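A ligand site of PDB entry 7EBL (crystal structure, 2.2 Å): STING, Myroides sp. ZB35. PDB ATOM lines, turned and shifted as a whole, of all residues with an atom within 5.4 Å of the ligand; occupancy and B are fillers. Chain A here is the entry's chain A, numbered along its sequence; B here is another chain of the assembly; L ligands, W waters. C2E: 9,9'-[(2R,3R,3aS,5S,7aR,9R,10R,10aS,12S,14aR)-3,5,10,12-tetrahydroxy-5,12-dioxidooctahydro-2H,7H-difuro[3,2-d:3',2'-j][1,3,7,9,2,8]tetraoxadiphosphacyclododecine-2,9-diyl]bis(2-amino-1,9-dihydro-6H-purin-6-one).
The side-chain amide nitrogen (ND2) of Asn 22 of chain A is in hydrogen-bond range of an oxygen (O11) of the ligand, at 2.6 Å. O2A of the ligand is in hydrogen-bond range of N of Thr 109 of chain A, at 3.2 Å. N of His 89 of chain B is in hydrogen-bond range of O6 of the ligand, at 3.2 Å. The backbone NH (N) of His 89 of chain A sits at hydrogen-bond distance from an oxygen (O61) of the ligand (3.1 Å). A nitrogen (N11) of the ligand sits at hydrogen-bond distance from the side-chain hydroxyl (OH) of Tyr 86 of chain B. A nitrogen (N71) of the ligand lies within hydrogen-bond range of the guanidinium group (NH1) of Arg 84 of chain A (2.9 Å). OD1 of Asp 105 of chain B sits at hydrogen-bond distance from N2 of the ligand, at 2.8 Å. O2' of the ligand lies within hydrogen-bond range of N of Thr 108 of chain B (3.4 Å). The side-chain hydroxyl of Tyr 86 of chain A lies close to a nitrogen (N3) of the ligand, at 3.3 Å. A nitrogen (N11) of the ligand lies within hydrogen-bond range of the backbone carbonyl oxygen (O) of His 89 of chain A, 2.4 Å away. The side-chain hydroxyl (OG1) of Thr 108 of chain A is in hydrogen-bond range of an oxygen (O2P) of the ligand (2.8 Å). The side-chain amide nitrogen of Asn 22 of chain B sits at hydrogen-bond distance from an oxygen (O1P) of the ligand (2.7 Å). N21 of the ligand sits at hydrogen-bond distance from OD1 of Asp 105 of chain A (2.7 Å). O2' of the ligand sits at hydrogen-bond distance from N of Thr 109 of chain B (3.3 Å). O of His 89 of chain B lies within hydrogen-bond range of N1 of the ligand. An oxygen (O6) of the ligand lies within hydrogen-bond range of the guanidinium group (NH2) of Arg 84 of chain B. An oxygen (O21) of the ligand lies within hydrogen-bond range of the side-chain hydroxyl of Thr 108 of chain B (2.8 Å).
A ring nitrogen (NE2) of His 89 of chain A sits at hydrogen-bond distance from a ring nitrogen (NE2) of His 89 of chain B, at 3.1 Å. The guanidinium group of Arg 84 of chain B is in hydrogen-bond range of the backbone carbonyl oxygen of Tyr 86 of chain B, at 3.0 Å. NH2 of Arg 84 of chain B is in hydrogen-bond range of O of Pro 87 of chain B, at 2.8 Å. The side-chain carboxylate (OD2) of Asp 105 of chain A lies within hydrogen-bond range of the side-chain hydroxyl (OH) of Tyr 19 of chain A, 2.7 Å away. The backbone carbonyl oxygen (O) of Pro 87 of chain A sits at hydrogen-bond distance from the guanidinium group (NH2) of Arg 84 of chain A, 2.9 Å away. OD2 of Asp 105 of chain B sits at hydrogen-bond distance from OH of Tyr 19 of chain B, 2.4 Å away. NE of Arg 84 of chain A lies within hydrogen-bond range of O of Tyr 86 of chain A, 3.0 Å away.
Tyr 19 of chain A touches the ligand (CD1 to O4A, 3.5 Å). Leu 23 of chain A touches the ligand (CD2 to N31, 3.3 Å). Ile 88 of chain A touches the ligand. CD1 of Tyr 19 of chain B touches O4' of the ligand (3.5 Å). CD1 of Leu 23 of chain B touches C5 of the ligand, 3.5 Å away. CA of Ile 88 of chain B touches O6 of the ligand, at 3.8 Å. Ile 90 of chain B touches the ligand (CG2 to N2, 3.99 Å). Hydrophobic or aromatic side chains within 4 Å of the ligand: Tyr 19 of chain A, Leu 23 of chain A, Tyr 86 of chain A, Tyr 19 of chain B, Leu 23 of chain B, Tyr 86 of chain B and Ile 90 of chain B. Within 4 Å of the ligand: Tyr 19 of chain A, Asn 22 of chain A, Leu 23 of chain A, Arg 84 of chain A, Tyr 86 of chain A, Ile 88 of chain A, His 89 of chain A, Asp 105 of chain A, Thr 108 of chain A, Thr 109 of chain A, Tyr 19 of chain B, Asn 22 of chain B, Leu 23 of chain B, Arg 84 of chain B, Tyr 86 of chain B, Ile 88 of chain B, His 89 of chain B, Ile 90 of chain B, Asp 105 of chain B, Thr 108 of chain B and Thr 109 of chain B. The nearest printed residue that does not touch the ligand is Gly 18 of chain B (4.1 Å).
Water W5 lies within hydrogen-bond range of O2P of the ligand, NH1 of Arg 84 of chain B and OG1 of Thr 108 of chain A. Water W4 lies within hydrogen-bond range of N31 of the ligand (2.8 Å), OD2 of Asp 105 of chain A (2.8 Å) and N of Thr 108 of chain A (3.2 Å). Water W7 lies within hydrogen-bond range of the guanidinium group (NH1) of Arg 84 of chain A (2.8 Å), an oxygen (O21) of the ligand (2.8 Å) and the backbone carbonyl oxygen (O) of Asn 22 of chain A (3.0 Å). Water W8 lies within hydrogen-bond range of the side-chain hydroxyl of Thr 109 of chain B (2.6 Å) and an oxygen (O11) of the ligand (2.8 Å). Water W1 bridges the side-chain hydroxyl (OG1) of Thr 109 of chain A (2.7 Å) and an oxygen (O1P) of the ligand (2.9 Å). Water W3 bridges OD1 of Asp 105 of chain A (2.6 Å) and N21 of the ligand (3.3 Å).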
ATOM      1  N   GLY A  18     -21.266 -13.501   9.146  1.00  0.00           N
ATOM      2  CA  GLY A  18     -21.687 -13.141   7.791  1.00  0.00           C
ATOM      3  C   GLY A  18     -21.931 -14.362   6.928  1.00  0.00           C
ATOM      4  O   GLY A  18     -22.921 -14.430   6.197  1.00  0.00           O
ATOM      5  N   TYR A  19     -21.040 -15.351   7.014  1.00  0.00           N
ATOM      6  CA  TYR A  19     -21.143 -16.539   6.192  1.00  0.00           C
ATOM      7  C   TYR A  19     -22.396 -17.351   6.524  1.00  0.00           C
ATOM      8  O   TYR A  19     -23.055 -17.881   5.624  1.00  0.00           O
ATOM      9  CB  TYR A  19     -19.882 -17.385   6.377  1.00  0.00           C
ATOM     10  CG  TYR A  19     -19.836 -18.609   5.504  1.00  0.00           C
ATOM     11  CD1 TYR A  19     -19.508 -18.507   4.164  1.00  0.00           C
ATOM     12  CD2 TYR A  19     -20.095 -19.864   6.035  1.00  0.00           C
ATOM     13  CE1 TYR A  19     -19.449 -19.627   3.368  1.00  0.00           C
ATOM     14  CE2 TYR A  19     -20.035 -20.983   5.240  1.00  0.00           C
ATOM     15  CZ  TYR A  19     -19.718 -20.861   3.907  1.00  0.00           C
ATOM     16  OH  TYR A  19     -19.670 -21.988   3.132  1.00  0.00           O
ATOM     17  N   ASN A  22     -25.649 -15.111   5.397  1.00  0.00           N
ATOM     18  CA  ASN A  22     -25.807 -14.760   3.999  1.00  0.00           C
ATOM     19  C   ASN A  22     -25.426 -15.894   3.053  1.00  0.00           C
ATOM     20  O   ASN A  22     -25.368 -15.672   1.840  1.00  0.00           O
ATOM     21  CB  ASN A  22     -24.971 -13.508   3.706  1.00  0.00           C
ATOM     22  CG  ASN A  22     -25.431 -12.309   4.517  1.00  0.00           C
ATOM     23  OD1 ASN A  22     -26.601 -12.211   4.893  1.00  0.00           O
ATOM     24  ND2 ASN A  22     -24.505 -11.388   4.792  1.00  0.00           N
ATOM     25  N   LEU A  23     -25.163 -17.086   3.559  1.00  0.00           N
ATOM     26  CA  LEU A  23     -25.028 -18.236   2.660  1.00  0.00           C
ATOM     27  C   LEU A  23     -25.660 -19.497   3.256  1.00  0.00           C
ATOM     28  O   LEU A  23     -26.533 -20.097   2.625  1.00  0.00           O
ATOM     29  CB  LEU A  23     -23.555 -18.489   2.298  1.00  0.00           C
ATOM     30  CG  LEU A  23     -23.289 -19.607   1.267  1.00  0.00           C
ATOM     31  CD1 LEU A  23     -24.051 -19.380  -0.041  1.00  0.00           C
ATOM     32  CD2 LEU A  23     -21.816 -19.853   0.997  1.00  0.00           C
ATOM     33  N   ARG A  84     -32.692 -13.558  -1.882  1.00  0.00           N
ATOM     34  CA  ARG A  84     -31.605 -12.758  -2.407  1.00  0.00           C
ATOM     35  C   ARG A  84     -31.891 -12.503  -3.882  1.00  0.00           C
ATOM     36  O   ARG A  84     -32.492 -13.329  -4.558  1.00  0.00           O
ATOM     37  CB  ARG A  84     -30.268 -13.494  -2.221  1.00  0.00           C
ATOM     38  CG  ARG A  84     -29.059 -12.772  -2.730  1.00  0.00           C
ATOM     39  CD  ARG A  84     -27.786 -13.436  -2.251  1.00  0.00           C
ATOM     40  NE  ARG A  84     -27.299 -14.510  -3.106  1.00  0.00           N
ATOM     41  CZ  ARG A  84     -26.198 -15.200  -2.858  1.00  0.00           C
ATOM     42  NH1 ARG A  84     -25.473 -14.976  -1.781  1.00  0.00           N
ATOM     43  NH2 ARG A  84     -25.794 -16.122  -3.742  1.00  0.00           N
ATOM     44  N   ASN A  85     -31.460 -11.335  -4.369  1.00  0.00           N
ATOM     45  CA  ASN A  85     -31.756 -10.989  -5.750  1.00  0.00           C
ATOM     46  C   ASN A  85     -30.819 -11.658  -6.762  1.00  0.00           C
ATOM     47  O   ASN A  85     -30.762 -11.222  -7.916  1.00  0.00           O
ATOM     48  CB  ASN A  85     -31.766  -9.469  -5.935  1.00  0.00           C
ATOM     49  CG  ASN A  85     -30.489  -8.820  -5.473  1.00  0.00           C
ATOM     50  OD1 ASN A  85     -29.462  -9.473  -5.315  1.00  0.00           O
ATOM     51  ND2 ASN A  85     -30.545  -7.511  -5.236  1.00  0.00           N
ATOM     52  N   TYR A  86     -30.042 -12.657  -6.349  1.00  0.00           N
ATOM     53  CA  TYR A  86     -29.301 -13.476  -7.301  1.00  0.00           C
ATOM     54  C   TYR A  86     -29.090 -14.864  -6.709  1.00  0.00           C
ATOM     55  O   TYR A  86     -29.059 -15.022  -5.482  1.00  0.00           O
ATOM     56  CB  TYR A  86     -27.957 -12.837  -7.681  1.00  0.00           C
ATOM     57  CG  TYR A  86     -27.015 -12.520  -6.554  1.00  0.00           C
ATOM     58  CD1 TYR A  86     -27.126 -11.329  -5.862  1.00  0.00           C
ATOM     59  CD2 TYR A  86     -25.997 -13.392  -6.211  1.00  0.00           C
ATOM     60  CE1 TYR A  86     -26.261 -11.014  -4.841  1.00  0.00           C
ATOM     61  CE2 TYR A  86     -25.121 -13.085  -5.192  1.00  0.00           C
ATOM     62  CZ  TYR A  86     -25.254 -11.900  -4.499  1.00  0.00           C
ATOM     63  OH  TYR A  86     -24.380 -11.584  -3.483  1.00  0.00           O
ATOM     64  N   PRO A  87     -28.988 -15.898  -7.551  1.00  0.00           N
ATOM     65  CA  PRO A  87     -28.983 -17.271  -7.026  1.00  0.00           C
ATOM     66  C   PRO A  87     -27.681 -17.615  -6.312  1.00  0.00           C
ATOM     67  O   PRO A  87     -26.662 -16.921  -6.404  1.00  0.00           O
ATOM     68  CB  PRO A  87     -29.176 -18.117  -8.279  1.00  0.00           C
ATOM     69  CG  PRO A  87     -28.682 -17.276  -9.395  1.00  0.00           C
ATOM     70  CD  PRO A  87     -29.008 -15.863  -9.012  1.00  0.00           C
ATOM     71  N   ILE A  88     -27.743 -18.726  -5.578  1.00  0.00           N
ATOM     72  CA  ILE A  88     -26.618 -19.294  -4.850  1.00  0.00           C
ATOM     73  C   ILE A  88     -25.775 -20.143  -5.788  1.00  0.00           C
ATOM     74  O   ILE A  88     -26.310 -20.921  -6.585  1.00  0.00           O
ATOM     75  CB  ILE A  88     -27.126 -20.144  -3.676  1.00  0.00           C
ATOM     76  CG1 ILE A  88     -27.945 -19.279  -2.710  1.00  0.00           C
ATOM     77  CG2 ILE A  88     -25.993 -20.884  -2.983  1.00  0.00           C
ATOM     78  CD1 ILE A  88     -28.887 -20.080  -1.836  1.00  0.00           C
ATOM     79  N   HIS A  89     -24.452 -20.018  -5.693  1.00  0.00           N
ATOM     80  CA  HIS A  89     -23.536 -20.815  -6.497  1.00  0.00           C
ATOM     81  C   HIS A  89     -22.620 -21.618  -5.583  1.00  0.00           C
ATOM     82  O   HIS A  89     -21.791 -21.037  -4.865  1.00  0.00           O
ATOM     83  CB  HIS A  89     -22.707 -19.919  -7.410  1.00  0.00           C
ATOM     84  CG  HIS A  89     -23.498 -19.273  -8.500  1.00  0.00           C
ATOM     85  ND1 HIS A  89     -23.719 -19.878  -9.717  1.00  0.00           N
ATOM     86  CD2 HIS A  89     -24.122 -18.076  -8.561  1.00  0.00           C
ATOM     87  CE1 HIS A  89     -24.446 -19.083 -10.488  1.00  0.00           C
ATOM     88  NE2 HIS A  89     -24.708 -17.983  -9.805  1.00  0.00           N
ATOM     89  N   ILE A  90     -22.758 -22.942  -5.608  1.00  0.00           N
ATOM     90  CA  ILE A  90     -21.869 -23.774  -4.798  1.00  0.00           C
ATOM     91  C   ILE A  90     -21.374 -24.939  -5.640  1.00  0.00           C
ATOM     92  O   ILE A  90     -21.426 -24.899  -6.876  1.00  0.00           O
ATOM     93  CB  ILE A  90     -22.568 -24.269  -3.519  1.00  0.00           C
ATOM     94  CG1 ILE A  90     -23.935 -24.854  -3.827  1.00  0.00           C
ATOM     95  CG2 ILE A  90     -22.705 -23.119  -2.513  1.00  0.00           C
ATOM     96  CD1 ILE A  90     -24.640 -25.381  -2.614  1.00  0.00           C
ATOM     97  N   ASP A 105     -18.919 -26.348  -0.098  1.00  0.00           N
ATOM     98  CA  ASP A 105     -18.350 -25.019  -0.270  1.00  0.00           C
ATOM     99  C   ASP A 105     -17.146 -24.866   0.635  1.00  0.00           C
ATOM    100  O   ASP A 105     -17.122 -25.412   1.741  1.00  0.00           O
ATOM    101  CB  ASP A 105     -19.351 -23.899   0.039  1.00  0.00           C
ATOM    102  CG  ASP A 105     -18.765 -22.510  -0.238  1.00  0.00           C
ATOM    103  OD1 ASP A 105     -18.425 -22.247  -1.419  1.00  0.00           O
ATOM    104  OD2 ASP A 105     -18.620 -21.706   0.712  1.00  0.00           O
ATOM    105  N   PRO A 107     -15.366 -21.695   2.390  1.00  0.00           N
ATOM    106  CA  PRO A 107     -15.724 -20.271   2.558  1.00  0.00           C
ATOM    107  C   PRO A 107     -14.656 -19.301   2.108  1.00  0.00           C
ATOM    108  O   PRO A 107     -13.606 -19.148   2.738  1.00  0.00           O
ATOM    109  CB  PRO A 107     -15.990 -20.140   4.062  1.00  0.00           C
ATOM    110  CG  PRO A 107     -16.219 -21.531   4.546  1.00  0.00           C
ATOM    111  CD  PRO A 107     -15.382 -22.416   3.675  1.00  0.00           C
ATOM    112  N   THR A 108     -14.928 -18.600   1.008  1.00  0.00           N
ATOM    113  CA  THR A 108     -13.950 -17.646   0.488  1.00  0.00           C
ATOM    114  C   THR A 108     -13.727 -16.489   1.447  1.00  0.00           C
ATOM    115  O   THR A 108     -12.606 -15.961   1.525  1.00  0.00           O
ATOM    116  CB  THR A 108     -14.424 -17.169  -0.895  1.00  0.00           C
ATOM    117  OG1 THR A 108     -15.757 -16.676  -0.810  1.00  0.00           O
ATOM    118  CG2 THR A 108     -14.446 -18.332  -1.859  1.00  0.00           C
ATOM    119  N   THR A 109     -14.752 -16.113   2.227  1.00  0.00           N
ATOM    120  CA  THR A 109     -14.629 -15.012   3.173  1.00  0.00           C
ATOM    121  C   THR A 109     -13.467 -15.216   4.161  1.00  0.00           C
ATOM    122  O   THR A 109     -12.880 -14.233   4.655  1.00  0.00           O
ATOM    123  CB  THR A 109     -15.969 -14.823   3.905  1.00  0.00           C
ATOM    124  OG1 THR A 109     -15.962 -13.630   4.697  1.00  0.00           O
ATOM    125  CG2 THR A 109     -16.301 -16.034   4.793  1.00  0.00           C
ATOM    126  N   GLY B  18     -12.951  -7.735   3.045  1.00  0.00           N
ATOM    127  CA  GLY B  18     -13.523  -8.828   2.285  1.00  0.00           C
ATOM    128  C   GLY B  18     -14.311  -8.364   1.062  1.00  0.00           C
ATOM    129  O   GLY B  18     -14.203  -8.947  -0.018  1.00  0.00           O
ATOM    130  N   TYR B  19     -15.101  -7.310   1.233  1.00  0.00           N
ATOM    131  CA  TYR B  19     -15.923  -6.797   0.133  1.00  0.00           C
ATOM    132  C   TYR B  19     -15.066  -6.254  -1.002  1.00  0.00           C
ATOM    133  O   TYR B  19     -15.369  -6.468  -2.179  1.00  0.00           O
ATOM    134  CB  TYR B  19     -16.870  -5.717   0.648  1.00  0.00           C
ATOM    135  CG  TYR B  19     -17.840  -5.184  -0.382  1.00  0.00           C
ATOM    136  CD1 TYR B  19     -18.989  -5.891  -0.699  1.00  0.00           C
ATOM    137  CD2 TYR B  19     -17.619  -3.966  -0.998  1.00  0.00           C
ATOM    138  CE1 TYR B  19     -19.896  -5.403  -1.619  1.00  0.00           C
ATOM    139  CE2 TYR B  19     -18.511  -3.467  -1.930  1.00  0.00           C
ATOM    140  CZ  TYR B  19     -19.655  -4.192  -2.241  1.00  0.00           C
ATOM    141  OH  TYR B  19     -20.544  -3.702  -3.170  1.00  0.00           O
ATOM    142  N   ASN B  22     -13.133  -9.469  -2.669  1.00  0.00           N
ATOM    143  CA  ASN B  22     -13.900 -10.537  -3.293  1.00  0.00           C
ATOM    144  C   ASN B  22     -15.088 -10.051  -4.122  1.00  0.00           C
ATOM    145  O   ASN B  22     -15.790 -10.879  -4.704  1.00  0.00           O
ATOM    146  CB  ASN B  22     -14.359 -11.533  -2.219  1.00  0.00           C
ATOM    147  CG  ASN B  22     -13.178 -12.233  -1.553  1.00  0.00           C
ATOM    148  OD1 ASN B  22     -12.145 -12.428  -2.179  1.00  0.00           O
ATOM    149  ND2 ASN B  22     -13.322 -12.583  -0.279  1.00  0.00           N
ATOM    150  N   LEU B  23     -15.331  -8.744  -4.202  1.00  0.00           N
ATOM    151  CA  LEU B  23     -16.303  -8.244  -5.158  1.00  0.00           C
ATOM    152  C   LEU B  23     -15.742  -7.079  -5.963  1.00  0.00           C
ATOM    153  O   LEU B  23     -15.729  -7.119  -7.205  1.00  0.00           O
ATOM    154  CB  LEU B  23     -17.603  -7.819  -4.477  1.00  0.00           C
ATOM    155  CG  LEU B  23     -18.621  -7.248  -5.479  1.00  0.00           C
ATOM    156  CD1 LEU B  23     -19.164  -8.328  -6.400  1.00  0.00           C
ATOM    157  CD2 LEU B  23     -19.748  -6.520  -4.798  1.00  0.00           C
ATOM    158  N   ARG B  84     -13.263 -16.617 -10.382  1.00  0.00           N
ATOM    159  CA  ARG B  84     -14.227 -17.262  -9.508  1.00  0.00           C
ATOM    160  C   ARG B  84     -15.066 -18.205 -10.368  1.00  0.00           C
ATOM    161  O   ARG B  84     -15.314 -17.922 -11.541  1.00  0.00           O
ATOM    162  CB  ARG B  84     -15.093 -16.218  -8.801  1.00  0.00           C
ATOM    163  CG  ARG B  84     -16.116 -16.765  -7.837  1.00  0.00           C
ATOM    164  CD  ARG B  84     -16.723 -15.665  -6.987  1.00  0.00           C
ATOM    165  NE  ARG B  84     -17.864 -15.022  -7.634  1.00  0.00           N
ATOM    166  CZ  ARG B  84     -18.584 -14.043  -7.106  1.00  0.00           C
ATOM    167  NH1 ARG B  84     -18.297 -13.554  -5.902  1.00  0.00           N
ATOM    168  NH2 ARG B  84     -19.637 -13.574  -7.763  1.00  0.00           N
ATOM    169  N   TYR B  86     -18.094 -18.744 -10.410  1.00  0.00           N
ATOM    170  CA  TYR B  86     -19.435 -18.291 -10.729  1.00  0.00           C
ATOM    171  C   TYR B  86     -19.385 -16.788 -10.957  1.00  0.00           C
ATOM    172  O   TYR B  86     -18.556 -16.092 -10.362  1.00  0.00           O
ATOM    173  CB  TYR B  86     -20.458 -18.637  -9.642  1.00  0.00           C
ATOM    174  CG  TYR B  86     -20.210 -18.092  -8.256  1.00  0.00           C
ATOM    175  CD1 TYR B  86     -19.389 -18.765  -7.357  1.00  0.00           C
ATOM    176  CD2 TYR B  86     -20.847 -16.932  -7.822  1.00  0.00           C
ATOM    177  CE1 TYR B  86     -19.183 -18.275  -6.070  1.00  0.00           C
ATOM    178  CE2 TYR B  86     -20.645 -16.445  -6.543  1.00  0.00           C
ATOM    179  CZ  TYR B  86     -19.805 -17.122  -5.675  1.00  0.00           C
ATOM    180  OH  TYR B  86     -19.606 -16.626  -4.399  1.00  0.00           O
ATOM    181  N   PRO B  87     -20.248 -16.271 -11.827  1.00  0.00           N
ATOM    182  CA  PRO B  87     -20.136 -14.868 -12.228  1.00  0.00           C
ATOM    183  C   PRO B  87     -20.551 -13.906 -11.132  1.00  0.00           C
ATOM    184  O   PRO B  87     -21.106 -14.277 -10.090  1.00  0.00           O
ATOM    185  CB  PRO B  87     -21.085 -14.773 -13.428  1.00  0.00           C
ATOM    186  CG  PRO B  87     -22.061 -15.893 -13.238  1.00  0.00           C
ATOM    187  CD  PRO B  87     -21.284 -16.994 -12.590  1.00  0.00           C
ATOM    188  N   ILE B  88     -20.235 -12.642 -11.373  1.00  0.00           N
ATOM    189  CA  ILE B  88     -20.623 -11.554 -10.498  1.00  0.00           C
ATOM    190  C   ILE B  88     -22.064 -11.173 -10.812  1.00  0.00           C
ATOM    191  O   ILE B  88     -22.429 -10.999 -11.978  1.00  0.00           O
ATOM    192  CB  ILE B  88     -19.691 -10.355 -10.705  1.00  0.00           C
ATOM    193  CG1 ILE B  88     -18.245 -10.771 -10.438  1.00  0.00           C
ATOM    194  CG2 ILE B  88     -20.118  -9.183  -9.838  1.00  0.00           C
ATOM    195  CD1 ILE B  88     -17.242  -9.887 -11.104  1.00  0.00           C
ATOM    196  N   HIS B  89     -22.876 -10.993  -9.781  1.00  0.00           N
ATOM    197  CA  HIS B  89     -24.266 -10.595  -9.947  1.00  0.00           C
ATOM    198  C   HIS B  89     -24.433  -9.235  -9.292  1.00  0.00           C
ATOM    199  O   HIS B  89     -24.331  -9.111  -8.068  1.00  0.00           O
ATOM    200  CB  HIS B  89     -25.225 -11.600  -9.294  1.00  0.00           C
ATOM    201  CG  HIS B  89     -25.300 -12.931  -9.971  1.00  0.00           C
ATOM    202  ND1 HIS B  89     -26.147 -13.185 -11.027  1.00  0.00           N
ATOM    203  CD2 HIS B  89     -24.689 -14.107  -9.688  1.00  0.00           C
ATOM    204  CE1 HIS B  89     -26.028 -14.449 -11.395  1.00  0.00           C
ATOM    205  NE2 HIS B  89     -25.146 -15.037 -10.596  1.00  0.00           N
ATOM    206  N   ILE B  90     -24.704  -8.204 -10.101  1.00  0.00           N
ATOM    207  CA  ILE B  90     -24.944  -6.887  -9.513  1.00  0.00           C
ATOM    208  C   ILE B  90     -26.162  -6.253 -10.181  1.00  0.00           C
ATOM    209  O   ILE B  90     -26.930  -6.927 -10.872  1.00  0.00           O
ATOM    210  CB  ILE B  90     -23.705  -5.972  -9.601  1.00  0.00           C
ATOM    211  CG1 ILE B  90     -23.108  -5.982 -11.001  1.00  0.00           C
ATOM    212  CG2 ILE B  90     -22.659  -6.382  -8.565  1.00  0.00           C
ATOM    213  CD1 ILE B  90     -21.909  -5.079 -11.125  1.00  0.00           C
ATOM    214  N   ASP B 105     -24.314  -1.541  -6.207  1.00  0.00           N
ATOM    215  CA  ASP B 105     -24.467  -2.582  -5.190  1.00  0.00           C
ATOM    216  C   ASP B 105     -24.594  -1.939  -3.822  1.00  0.00           C
ATOM    217  O   ASP B 105     -23.947  -0.924  -3.534  1.00  0.00           O
ATOM    218  CB  ASP B 105     -23.296  -3.569  -5.197  1.00  0.00           C
ATOM    219  CG  ASP B 105     -23.505  -4.724  -4.211  1.00  0.00           C
ATOM    220  OD1 ASP B 105     -24.497  -5.475  -4.366  1.00  0.00           O
ATOM    221  OD2 ASP B 105     -22.687  -4.876  -3.282  1.00  0.00           O
ATOM    222  N   PRO B 107     -23.725  -3.275  -0.130  1.00  0.00           N
ATOM    223  CA  PRO B 107     -23.011  -4.462   0.371  1.00  0.00           C
ATOM    224  C   PRO B 107     -23.773  -5.240   1.426  1.00  0.00           C
ATOM    225  O   PRO B 107     -23.937  -4.778   2.561  1.00  0.00           O
ATOM    226  CB  PRO B 107     -21.724  -3.866   0.970  1.00  0.00           C
ATOM    227  CG  PRO B 107     -21.592  -2.517   0.372  1.00  0.00           C
ATOM    228  CD  PRO B 107     -22.996  -2.034   0.139  1.00  0.00           C
ATOM    229  N   THR B 108     -24.219  -6.452   1.077  1.00  0.00           N
ATOM    230  CA  THR B 108     -24.998  -7.246   2.028  1.00  0.00           C
ATOM    231  C   THR B 108     -24.171  -7.653   3.256  1.00  0.00           C
ATOM    232  O   THR B 108     -24.731  -7.813   4.348  1.00  0.00           O
ATOM    233  CB  THR B 108     -25.615  -8.451   1.303  1.00  0.00           C
ATOM    234  OG1 THR B 108     -24.598  -9.173   0.609  1.00  0.00           O
ATOM    235  CG2 THR B 108     -26.654  -7.986   0.298  1.00  0.00           C
ATOM    236  N   THR B 109     -22.841  -7.795   3.111  1.00  0.00           N
ATOM    237  CA  THR B 109     -21.986  -8.150   4.232  1.00  0.00           C
ATOM    238  C   THR B 109     -22.165  -7.204   5.430  1.00  0.00           C
ATOM    239  O   THR B 109     -22.030  -7.625   6.586  1.00  0.00           O
ATOM    240  CB  THR B 109     -20.522  -8.164   3.768  1.00  0.00           C
ATOM    241  OG1 THR B 109     -19.671  -8.704   4.785  1.00  0.00           O
ATOM    242  CG2 THR B 109     -20.038  -6.755   3.410  1.00  0.00           C
HETATM  243  P1  C2E L   1     -17.133 -13.191   0.121  1.00  0.00           P
HETATM  244  O2P C2E L   1     -16.804 -14.045  -1.068  1.00  0.00           O
HETATM  245  O1P C2E L   1     -15.817 -12.635   0.630  1.00  0.00           O
HETATM  246  O5' C2E L   1     -18.029 -11.880  -0.259  1.00  0.00           O
HETATM  247  C5' C2E L   1     -17.891 -10.780   0.563  1.00  0.00           C
HETATM  248  C4' C2E L   1     -19.079  -9.834   0.240  1.00  0.00           C
HETATM  249  O4' C2E L   1     -18.943  -9.383  -0.979  1.00  0.00           O
HETATM  250  C3' C2E L   1     -20.417 -10.591   0.267  1.00  0.00           C
HETATM  251  O3' C2E L   1     -20.877 -10.568   1.541  1.00  0.00           O
HETATM  252  C2' C2E L   1     -21.259  -9.691  -0.652  1.00  0.00           C
HETATM  253  O2' C2E L   1     -21.651  -8.473   0.119  1.00  0.00           O
HETATM  254  C1' C2E L   1     -20.431  -9.319  -1.604  1.00  0.00           C
HETATM  255  N9  C2E L   1     -20.443 -10.126  -2.802  1.00  0.00           N
HETATM  256  C8  C2E L   1     -19.586 -11.114  -3.069  1.00  0.00           C
HETATM  257  N7  C2E L   1     -19.967 -11.572  -4.291  1.00  0.00           N
HETATM  258  C5  C2E L   1     -21.011 -10.858  -4.730  1.00  0.00           C
HETATM  259  C6  C2E L   1     -21.848 -10.897  -6.015  1.00  0.00           C
HETATM  260  O6  C2E L   1     -21.628 -11.680  -6.867  1.00  0.00           O
HETATM  261  N1  C2E L   1     -22.920  -9.966  -6.183  1.00  0.00           N
HETATM  262  C2  C2E L   1     -23.225  -9.004  -5.160  1.00  0.00           C
HETATM  263  N2  C2E L   1     -24.306  -8.058  -5.341  1.00  0.00           N
HETATM  264  N3  C2E L   1     -22.422  -8.963  -3.941  1.00  0.00           N
HETATM  265  C4  C2E L   1     -21.313  -9.927  -3.777  1.00  0.00           C
HETATM  266  P11 C2E L   1     -22.008 -11.726   1.901  1.00  0.00           P
HETATM  267  O21 C2E L   1     -23.350 -11.624   1.218  1.00  0.00           O
HETATM  268  O11 C2E L   1     -22.306 -11.507   3.369  1.00  0.00           O
HETATM  269  O5A C2E L   1     -21.282 -13.183   1.689  1.00  0.00           O
HETATM  270  C5A C2E L   1     -20.637 -13.696   2.821  1.00  0.00           C
HETATM  271  C4A C2E L   1     -19.911 -14.920   2.410  1.00  0.00           C
HETATM  272  O4A C2E L   1     -20.743 -15.891   2.127  1.00  0.00           O
HETATM  273  C3A C2E L   1     -19.050 -14.655   1.006  1.00  0.00           C
HETATM  274  O3A C2E L   1     -17.760 -14.023   1.399  1.00  0.00           O
HETATM  275  C2A C2E L   1     -18.875 -15.774   0.525  1.00  0.00           C
HETATM  276  O2A C2E L   1     -17.763 -16.519   1.219  1.00  0.00           O
HETATM  277  C1A C2E L   1     -20.235 -16.569   0.874  1.00  0.00           C
HETATM  278  N91 C2E L   1     -21.146 -16.532  -0.092  1.00  0.00           N
HETATM  279  C81 C2E L   1     -22.219 -15.736  -0.235  1.00  0.00           C
HETATM  280  N71 C2E L   1     -22.835 -16.116  -1.362  1.00  0.00           N
HETATM  281  C51 C2E L   1     -22.175 -17.130  -1.908  1.00  0.00           C
HETATM  282  C61 C2E L   1     -22.430 -17.953  -3.166  1.00  0.00           C
HETATM  283  O61 C2E L   1     -23.365 -17.731  -3.861  1.00  0.00           O
HETATM  284  N11 C2E L   1     -21.535 -19.018  -3.511  1.00  0.00           N
HETATM  285  C21 C2E L   1     -20.406 -19.301  -2.675  1.00  0.00           C
HETATM  286  N21 C2E L   1     -19.489 -20.373  -3.026  1.00  0.00           N
HETATM  287  N31 C2E L   1     -20.185 -18.505  -1.471  1.00  0.00           N
HETATM  288  C41 C2E L   1     -21.111 -17.400  -1.107  1.00  0.00           C
HETATM  289  O   HOH W   1     -15.463 -11.365   3.243  1.00  0.00           O
HETATM  290  O   HOH W   2     -23.366  -7.138  -1.890  1.00  0.00           O
HETATM  291  O   HOH W   3     -18.802 -23.542  -3.597  1.00  0.00           O
HETATM  292  O   HOH W   4     -17.935 -19.066   0.013  1.00  0.00           O
HETATM  293  O   HOH W   5     -16.455 -14.752  -3.609  1.00  0.00           O
HETATM  294  O   HOH W   6     -17.060  -9.057   3.435  1.00  0.00           O
HETATM  295  O   HOH W   7     -25.517 -13.128   0.306  1.00  0.00           O
HETATM  296  O   HOH W   8     -20.376 -11.143   5.415  1.00  0.00           O
